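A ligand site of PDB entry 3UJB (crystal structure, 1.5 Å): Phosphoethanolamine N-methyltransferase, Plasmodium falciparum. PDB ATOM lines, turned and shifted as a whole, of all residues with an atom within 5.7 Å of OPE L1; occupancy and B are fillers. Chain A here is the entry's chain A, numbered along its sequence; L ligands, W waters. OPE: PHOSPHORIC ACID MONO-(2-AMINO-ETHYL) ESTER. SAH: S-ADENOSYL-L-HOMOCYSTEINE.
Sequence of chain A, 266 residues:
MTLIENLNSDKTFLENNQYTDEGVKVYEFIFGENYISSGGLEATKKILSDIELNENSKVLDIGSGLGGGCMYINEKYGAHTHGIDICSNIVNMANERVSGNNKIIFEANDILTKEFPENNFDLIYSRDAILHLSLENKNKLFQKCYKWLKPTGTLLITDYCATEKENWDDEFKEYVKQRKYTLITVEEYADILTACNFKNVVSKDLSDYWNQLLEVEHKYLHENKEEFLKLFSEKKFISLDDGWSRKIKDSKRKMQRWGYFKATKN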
ATOM      1  N   GLN A  18      26.978   4.672   2.440  1.00  0.00           N
ATOM      2  CA  GLN A  18      25.876   3.725   2.547  1.00  0.00           C
ATOM      3  C   GLN A  18      25.126   3.516   1.239  1.00  0.00           C
ATOM      4  O   GLN A  18      24.694   2.406   0.940  1.00  0.00           O
ATOM      5  CB  GLN A  18      24.896   4.159   3.625  1.00  0.00           C
ATOM      6  CG  GLN A  18      23.794   3.132   3.875  1.00  0.00           C
ATOM      7  CD  GLN A  18      22.943   3.447   5.082  1.00  0.00           C
ATOM      8  OE1 GLN A  18      22.968   4.558   5.613  1.00  0.00           O
ATOM      9  NE2 GLN A  18      22.179   2.461   5.535  1.00  0.00           N
ATOM     10  N   TYR A  19      24.967   4.587   0.458  1.00  0.00           N
ATOM     11  CA  TYR A  19      24.203   4.491  -0.774  1.00  0.00           C
ATOM     12  C   TYR A  19      25.017   4.768  -2.040  1.00  0.00           C
ATOM     13  O   TYR A  19      24.565   5.477  -2.940  1.00  0.00           O
ATOM     14  CB  TYR A  19      22.963   5.384  -0.717  1.00  0.00           C
ATOM     15  CG  TYR A  19      22.069   5.139   0.488  1.00  0.00           C
ATOM     16  CD1 TYR A  19      21.374   3.940   0.632  1.00  0.00           C
ATOM     17  CD2 TYR A  19      21.906   6.109   1.452  1.00  0.00           C
ATOM     18  CE1 TYR A  19      20.549   3.715   1.724  1.00  0.00           C
ATOM     19  CE2 TYR A  19      21.081   5.894   2.554  1.00  0.00           C
ATOM     20  CZ  TYR A  19      20.409   4.701   2.681  1.00  0.00           C
ATOM     21  OH  TYR A  19      19.589   4.516   3.783  1.00  0.00           O
ATOM     22  N   TYR A  27      21.433  -3.642  -1.286  1.00  0.00           N
ATOM     23  CA  TYR A  27      20.204  -3.506  -0.525  1.00  0.00           C
ATOM     24  C   TYR A  27      18.994  -3.977  -1.329  1.00  0.00           C
ATOM     25  O   TYR A  27      18.106  -4.641  -0.809  1.00  0.00           O
ATOM     26  CB  TYR A  27      20.018  -2.050  -0.089  1.00  0.00           C
ATOM     27  CG  TYR A  27      20.762  -1.648   1.173  1.00  0.00           C
ATOM     28  CD1 TYR A  27      20.762  -2.461   2.302  1.00  0.00           C
ATOM     29  CD2 TYR A  27      21.454  -0.437   1.230  1.00  0.00           C
ATOM     30  CE1 TYR A  27      21.424  -2.078   3.463  1.00  0.00           C
ATOM     31  CE2 TYR A  27      22.127  -0.055   2.383  1.00  0.00           C
ATOM     32  CZ  TYR A  27      22.099  -0.874   3.488  1.00  0.00           C
ATOM     33  OH  TYR A  27      22.743  -0.479   4.647  1.00  0.00           O
ATOM     34  N   PHE A  31      16.147  -6.600  -0.108  1.00  0.00           N
ATOM     35  CA  PHE A  31      14.844  -6.030   0.220  1.00  0.00           C
ATOM     36  C   PHE A  31      13.797  -6.315  -0.851  1.00  0.00           C
ATOM     37  O   PHE A  31      12.607  -6.409  -0.573  1.00  0.00           O
ATOM     38  CB  PHE A  31      14.951  -4.508   0.429  1.00  0.00           C
ATOM     39  CG  PHE A  31      15.613  -4.094   1.711  1.00  0.00           C
ATOM     40  CD1 PHE A  31      15.159  -4.586   2.936  1.00  0.00           C
ATOM     41  CD2 PHE A  31      16.665  -3.189   1.699  1.00  0.00           C
ATOM     42  CE1 PHE A  31      15.753  -4.172   4.109  1.00  0.00           C
ATOM     43  CE2 PHE A  31      17.267  -2.787   2.883  1.00  0.00           C
ATOM     44  CZ  PHE A  31      16.805  -3.278   4.087  1.00  0.00           C
ATOM     45  N   ILE A  36      14.764  -0.262  -0.997  1.00  0.00           N
ATOM     46  CA  ILE A  36      15.965  -0.325  -0.180  1.00  0.00           C
ATOM     47  C   ILE A  36      15.631  -0.136   1.296  1.00  0.00           C
ATOM     48  O   ILE A  36      16.421   0.428   2.066  1.00  0.00           O
ATOM     49  CB  ILE A  36      17.074   0.640  -0.640  1.00  0.00           C
ATOM     50  CG1 ILE A  36      16.545   2.073  -0.740  1.00  0.00           C
ATOM     51  CG2 ILE A  36      17.630   0.196  -2.002  1.00  0.00           C
ATOM     52  CD1 ILE A  36      17.561   3.030  -1.363  1.00  0.00           C
ATOM     53  N   SER A  37      14.450  -0.615   1.684  1.00  0.00           N
ATOM     54  CA  SER A  37      14.104  -0.637   3.093  1.00  0.00           C
ATOM     55  C   SER A  37      13.255  -1.843   3.470  1.00  0.00           C
ATOM     56  O   SER A  37      12.704  -2.534   2.602  1.00  0.00           O
ATOM     57  CB  SER A  37      13.375   0.637   3.496  1.00  0.00           C
ATOM     58  OG  SER A  37      12.019   0.564   3.098  1.00  0.00           O
ATOM     59  N   ASP A 128      11.589   4.508   6.488  1.00  0.00           N
ATOM     60  CA  ASP A 128      12.980   4.304   6.928  1.00  0.00           C
ATOM     61  C   ASP A 128      13.934   5.311   6.296  1.00  0.00           C
ATOM     62  O   ASP A 128      14.995   4.938   5.772  1.00  0.00           O
ATOM     63  CB  ASP A 128      13.453   2.867   6.668  1.00  0.00           C
ATOM     64  CG  ASP A 128      12.587   1.817   7.362  1.00  0.00           C
ATOM     65  OD1 ASP A 128      11.711   2.184   8.181  1.00  0.00           O
ATOM     66  OD2 ASP A 128      12.810   0.619   7.096  1.00  0.00           O
ATOM     67  N   LEU A 131      15.499   8.475   9.993  1.00  0.00           N
ATOM     68  CA  LEU A 131      16.637   8.098  10.860  1.00  0.00           C
ATOM     69  C   LEU A 131      17.944   8.811  10.471  1.00  0.00           C
ATOM     70  O   LEU A 131      18.856   8.932  11.287  1.00  0.00           O
ATOM     71  CB  LEU A 131      16.874   6.576  10.825  1.00  0.00           C
ATOM     72  CG  LEU A 131      17.435   5.960   9.549  1.00  0.00           C
ATOM     73  CD1 LEU A 131      17.687   4.488   9.776  1.00  0.00           C
ATOM     74  CD2 LEU A 131      16.473   6.157   8.376  1.00  0.00           C
ATOM     75  N   HIS A 132      18.037   9.255   9.222  1.00  0.00           N
ATOM     76  CA  HIS A 132      19.204   9.989   8.755  1.00  0.00           C
ATOM     77  C   HIS A 132      19.281  11.406   9.315  1.00  0.00           C
ATOM     78  O   HIS A 132      20.344  12.036   9.301  1.00  0.00           O
ATOM     79  CB  HIS A 132      19.240  10.006   7.216  1.00  0.00           C
ATOM     80  CG  HIS A 132      19.525   8.656   6.609  1.00  0.00           C
ATOM     81  ND1 HIS A 132      20.737   8.021   6.755  1.00  0.00           N
ATOM     82  CD2 HIS A 132      18.757   7.846   5.858  1.00  0.00           C
ATOM     83  CE1 HIS A 132      20.698   6.861   6.112  1.00  0.00           C
ATOM     84  NE2 HIS A 132      19.506   6.732   5.564  1.00  0.00           N
ATOM     85  N   TYR A 160      13.453   3.542  11.752  1.00  0.00           N
ATOM     86  CA  TYR A 160      14.229   2.835  12.753  1.00  0.00           C
ATOM     87  C   TYR A 160      14.181   3.618  14.038  1.00  0.00           C
ATOM     88  O   TYR A 160      14.379   4.832  14.054  1.00  0.00           O
ATOM     89  CB  TYR A 160      15.689   2.686  12.323  1.00  0.00           C
ATOM     90  CG  TYR A 160      15.979   1.656  11.245  1.00  0.00           C
ATOM     91  CD1 TYR A 160      14.964   0.975  10.590  1.00  0.00           C
ATOM     92  CD2 TYR A 160      17.296   1.367  10.891  1.00  0.00           C
ATOM     93  CE1 TYR A 160      15.258   0.046   9.601  1.00  0.00           C
ATOM     94  CE2 TYR A 160      17.601   0.447   9.913  1.00  0.00           C
ATOM     95  CZ  TYR A 160      16.584  -0.224   9.278  1.00  0.00           C
ATOM     96  OH  TYR A 160      16.879  -1.143   8.299  1.00  0.00           O
ATOM     97  N   TYR A 175      27.357   0.632  15.355  1.00  0.00           N
ATOM     98  CA  TYR A 175      26.473   0.616  14.197  1.00  0.00           C
ATOM     99  C   TYR A 175      25.849   1.991  13.976  1.00  0.00           C
ATOM    100  O   TYR A 175      25.887   2.536  12.879  1.00  0.00           O
ATOM    101  CB  TYR A 175      25.390  -0.456  14.411  1.00  0.00           C
ATOM    102  CG  TYR A 175      24.161  -0.368  13.530  1.00  0.00           C
ATOM    103  CD1 TYR A 175      24.186  -0.794  12.203  1.00  0.00           C
ATOM    104  CD2 TYR A 175      22.950   0.088  14.044  1.00  0.00           C
ATOM    105  CE1 TYR A 175      23.033  -0.748  11.393  1.00  0.00           C
ATOM    106  CE2 TYR A 175      21.804   0.133  13.255  1.00  0.00           C
ATOM    107  CZ  TYR A 175      21.849  -0.286  11.940  1.00  0.00           C
ATOM    108  OH  TYR A 175      20.702  -0.240  11.162  1.00  0.00           O
ATOM    109  N   ARG A 179      26.763   4.517  10.874  1.00  0.00           N
ATOM    110  CA  ARG A 179      25.691   4.915   9.995  1.00  0.00           C
ATOM    111  C   ARG A 179      25.322   6.406  10.065  1.00  0.00           C
ATOM    112  O   ARG A 179      24.702   6.908   9.200  1.00  0.00           O
ATOM    113  CB  ARG A 179      24.428   4.073  10.292  1.00  0.00           C
ATOM    114  CG  ARG A 179      24.481   2.608   9.930  1.00  0.00           C
ATOM    115  CD  ARG A 179      24.414   2.347   8.477  1.00  0.00           C
ATOM    116  NE  ARG A 179      24.005   1.001   8.206  1.00  0.00           N
ATOM    117  CZ  ARG A 179      24.837  -0.033   8.153  1.00  0.00           C
ATOM    118  NH1 ARG A 179      26.125   0.160   8.339  1.00  0.00           N
ATOM    119  NH2 ARG A 179      24.377  -1.240   7.883  1.00  0.00           N
ATOM    120  N   TYR A 181      23.222   7.539  12.105  1.00  0.00           N
ATOM    121  CA  TYR A 181      21.789   7.602  12.389  1.00  0.00           C
ATOM    122  C   TYR A 181      21.562   8.360  13.683  1.00  0.00           C
ATOM    123  O   TYR A 181      22.408   8.371  14.574  1.00  0.00           O
ATOM    124  CB  TYR A 181      21.256   6.196  12.618  1.00  0.00           C
ATOM    125  CG  TYR A 181      21.152   5.295  11.428  1.00  0.00           C
ATOM    126  CD1 TYR A 181      21.158   5.793  10.126  1.00  0.00           C
ATOM    127  CD2 TYR A 181      21.037   3.918  11.608  1.00  0.00           C
ATOM    128  CE1 TYR A 181      21.058   4.942   9.046  1.00  0.00           C
ATOM    129  CE2 TYR A 181      20.926   3.069  10.536  1.00  0.00           C
ATOM    130  CZ  TYR A 181      20.931   3.587   9.264  1.00  0.00           C
ATOM    131  OH  TYR A 181      20.826   2.718   8.203  1.00  0.00           O
ATOM    132  N   TRP A 210       8.920  -6.619  12.319  1.00  0.00           N
ATOM    133  CA  TRP A 210      10.198  -6.307  11.684  1.00  0.00           C
ATOM    134  C   TRP A 210      11.143  -7.499  11.760  1.00  0.00           C
ATOM    135  O   TRP A 210      11.787  -7.853  10.780  1.00  0.00           O
ATOM    136  CB  TRP A 210      10.838  -5.074  12.339  1.00  0.00           C
ATOM    137  CG  TRP A 210      11.997  -4.503  11.583  1.00  0.00           C
ATOM    138  CD1 TRP A 210      12.017  -4.129  10.266  1.00  0.00           C
ATOM    139  CD2 TRP A 210      13.289  -4.207  12.099  1.00  0.00           C
ATOM    140  NE1 TRP A 210      13.255  -3.627   9.934  1.00  0.00           N
ATOM    141  CE2 TRP A 210      14.053  -3.669  11.052  1.00  0.00           C
ATOM    142  CE3 TRP A 210      13.881  -4.349  13.365  1.00  0.00           C
ATOM    143  CZ2 TRP A 210      15.384  -3.280  11.218  1.00  0.00           C
ATOM    144  CZ3 TRP A 210      15.202  -3.958  13.530  1.00  0.00           C
ATOM    145  CH2 TRP A 210      15.936  -3.426  12.470  1.00  0.00           C
ATOM    146  N   TRP A 244      22.393  -8.360   8.925  1.00  0.00           N
ATOM    147  CA  TRP A 244      21.037  -8.834   9.181  1.00  0.00           C
ATOM    148  C   TRP A 244      20.996  -9.650  10.466  1.00  0.00           C
ATOM    149  O   TRP A 244      20.039  -9.534  11.231  1.00  0.00           O
ATOM    150  CB  TRP A 244      20.480  -9.637   7.982  1.00  0.00           C
ATOM    151  CG  TRP A 244      19.487  -8.857   7.175  1.00  0.00           C
ATOM    152  CD1 TRP A 244      18.174  -9.148   6.978  1.00  0.00           C
ATOM    153  CD2 TRP A 244      19.741  -7.645   6.432  1.00  0.00           C
ATOM    154  NE1 TRP A 244      17.581  -8.205   6.177  1.00  0.00           N
ATOM    155  CE2 TRP A 244      18.519  -7.264   5.827  1.00  0.00           C
ATOM    156  CE3 TRP A 244      20.864  -6.843   6.229  1.00  0.00           C
ATOM    157  CZ2 TRP A 244      18.402  -6.129   5.029  1.00  0.00           C
ATOM    158  CZ3 TRP A 244      20.736  -5.706   5.440  1.00  0.00           C
ATOM    159  CH2 TRP A 244      19.517  -5.366   4.847  1.00  0.00           C
ATOM    160  N   LYS A 247      20.651  -7.248  13.319  1.00  0.00           N
ATOM    161  CA  LYS A 247      19.325  -6.645  13.392  1.00  0.00           C
ATOM    162  C   LYS A 247      18.323  -7.636  13.946  1.00  0.00           C
ATOM    163  O   LYS A 247      17.416  -7.264  14.691  1.00  0.00           O
ATOM    164  CB  LYS A 247      18.875  -6.111  12.033  1.00  0.00           C
ATOM    165  CG  LYS A 247      19.604  -4.847  11.619  1.00  0.00           C
ATOM    166  CD  LYS A 247      19.047  -4.225  10.326  1.00  0.00           C
ATOM    167  CE  LYS A 247      19.454  -5.020   9.085  1.00  0.00           C
ATOM    168  NZ  LYS A 247      18.915  -4.360   7.853  1.00  0.00           N
ATOM    169  N   GLN A 256      17.203  -2.477  19.036  1.00  0.00           N
ATOM    170  CA  GLN A 256      16.844  -1.753  17.824  1.00  0.00           C
ATOM    171  C   GLN A 256      15.366  -2.050  17.567  1.00  0.00           C
ATOM    172  O   GLN A 256      14.940  -3.209  17.643  1.00  0.00           O
ATOM    173  CB  GLN A 256      17.717  -2.193  16.623  1.00  0.00           C
ATOM    174  CG  GLN A 256      17.463  -1.353  15.362  1.00  0.00           C
ATOM    175  CD  GLN A 256      18.489  -1.562  14.265  1.00  0.00           C
ATOM    176  OE1 GLN A 256      19.448  -2.321  14.412  1.00  0.00           O
ATOM    177  NE2 GLN A 256      18.298  -0.862  13.146  1.00  0.00           N
HETATM  178  CA  OPE L   1      18.936  -0.069   5.565  1.00  0.00           C
HETATM  179  CB  OPE L   1      18.731   0.845   4.409  1.00  0.00           C
HETATM  180  O1  OPE L   1      21.668  -1.530   6.817  1.00  0.00           O
HETATM  181  O2  OPE L   1      19.421  -1.635   7.851  1.00  0.00           O
HETATM  182  O3  OPE L   1      21.026   0.142   8.592  1.00  0.00           O
HETATM  183  O4  OPE L   1      19.993   0.264   6.374  1.00  0.00           O
HETATM  184  N   OPE L   1      18.973   2.226   4.668  1.00  0.00           N
HETATM  185  P   OPE L   1      20.544  -0.722   7.454  1.00  0.00           P
HETATM  186  N   SAH L   2      11.823   4.870   1.257  1.00  0.00           N
HETATM  187  CA  SAH L   2      12.695   4.108   0.325  1.00  0.00           C
HETATM  188  CB  SAH L   2      14.208   4.440   0.596  1.00  0.00           C
HETATM  189  CG  SAH L   2      14.695   3.971   1.978  1.00  0.00           C
HETATM  190  SD  SAH L   2      16.460   4.306   2.270  1.00  0.00           S
HETATM  191  C   SAH L   2      12.378   2.679   0.431  1.00  0.00           C
HETATM  192  O   SAH L   2      11.646   2.288   1.317  1.00  0.00           O
HETATM  193  OXT SAH L   2      12.916   1.888  -0.310  1.00  0.00           O
HETATM  194  C5' SAH L   2      16.541   6.026   2.833  1.00  0.00           C
HETATM  195  C4' SAH L   2      16.495   7.069   1.855  1.00  0.00           C
HETATM  196  O4' SAH L   2      16.418   8.328   2.561  1.00  0.00           O
HETATM  197  C3' SAH L   2      17.745   7.111   1.052  1.00  0.00           C
HETATM  198  O3' SAH L   2      17.447   6.875  -0.320  1.00  0.00           O
HETATM  199  C2' SAH L   2      18.308   8.454   1.312  1.00  0.00           C
HETATM  200  O2' SAH L   2      18.956   9.049   0.199  1.00  0.00           O
HETATM  201  C1' SAH L   2      17.123   9.240   1.770  1.00  0.00           C
HETATM  202  N9  SAH L   2      17.453  10.489   2.548  1.00  0.00           N
HETATM  203  C8  SAH L   2      18.271  10.595   3.604  1.00  0.00           C
HETATM  204  N7  SAH L   2      18.277  11.870   3.998  1.00  0.00           N
HETATM  205  C5  SAH L   2      17.453  12.575   3.213  1.00  0.00           C
HETATM  206  C6  SAH L   2      17.091  13.933   3.156  1.00  0.00           C
HETATM  207  N6  SAH L   2      17.590  14.844   4.053  1.00  0.00           N
HETATM  208  N1  SAH L   2      16.221  14.320   2.202  1.00  0.00           N
HETATM  209  C2  SAH L   2      15.726  13.449   1.314  1.00  0.00           C
HETATM  210  N3  SAH L   2      16.058  12.136   1.337  1.00  0.00           N
HETATM  211  C4  SAH L   2      16.923  11.688   2.262  1.00  0.00           C
HETATM  212  O   HOH W   1      17.323   3.752   5.797  1.00  0.00           O
HETATM  213  O   HOH W   2      22.406  -3.949   7.965  1.00  0.00           O
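N of OPE L1 sits at hydrogen-bond distance from OH of Tyr 19 (2.5 Å).
OH of Tyr 181 sits at hydrogen-bond distance from O3 of OPE L1, at 2.6 Å.
O3 of OPE L1 sits at hydrogen-bond distance from OH of Tyr 175 (2.6 Å).
The side-chain hydroxyl of Tyr 160 sits at hydrogen-bond distance from an oxygen (O2) of OPE L1 (2.6 Å).
O1 of OPE L1 sits at hydrogen-bond distance from OH of Tyr 27 (2.6 Å).
The side-chain amino group (NZ) of Lys 247 lies within salt-bridge range of an oxygen (O2) of OPE L1, at 2.8 Å.
The guanidinium group of Arg 179 lies within salt-bridge range of an oxygen (O1) of OPE L1.
An oxygen (O4) of OPE L1 lies within hydrogen-bond range of the side-chain amide nitrogen of Gln 18 (3.2 Å).
OH of Tyr 19 sits close to SD of SAH L2 (3.5 Å).
The backbone NH of Ile 36 sits at hydrogen-bond distance from an oxygen (OXT) of SAH L2 (2.9 Å).
OG of Ser 37 sits at hydrogen-bond distance from O of SAH L2, 2.5 Å away.
A ring nitrogen (NE2) of His 132 lies within hydrogen-bond range of the side-chain hydroxyl (OH) of Tyr 19, at 2.8 Å.
The side-chain hydroxyl of Tyr 181 lies within hydrogen-bond range of the side-chain amide nitrogen of Gln 18 (3.0 Å).
The side-chain amide nitrogen (NE2) of Gln 256 sits at hydrogen-bond distance from the side-chain hydroxyl (OH) of Tyr 175 (3.2 Å).
The side-chain hydroxyl of Tyr 27 is in hydrogen-bond range of the side-chain amide nitrogen of Gln 18, 3.1 Å away.
Merely in contact with OPE L1: Ile 36 (3.3 Å).
Nine residues have an atom within 4 Å of OPE L1: Gln 18, Tyr 19, Tyr 27, Ile 36, Tyr 160, Tyr 175, Arg 179, Tyr 181 and Lys 247.
Along chain A the residues within 4 Å of OPE L1 span positions 18 to 247.
Water W1 lies within hydrogen-bond range of a nitrogen (N) of OPE L1 (2.5 Å), the backbone carbonyl oxygen (O) of Asp 128 (2.6 Å), the side-chain hydroxyl (OH) of Tyr 19 (3.1 Å) and a sulfur (SD) of SAH L2 (3.7 Å).
Water W2 lies within hydrogen-bond range of an oxygen (O1) of OPE L1 (2.8 Å) and the guanidinium group (NH2) of Arg 179 (3.4 Å).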
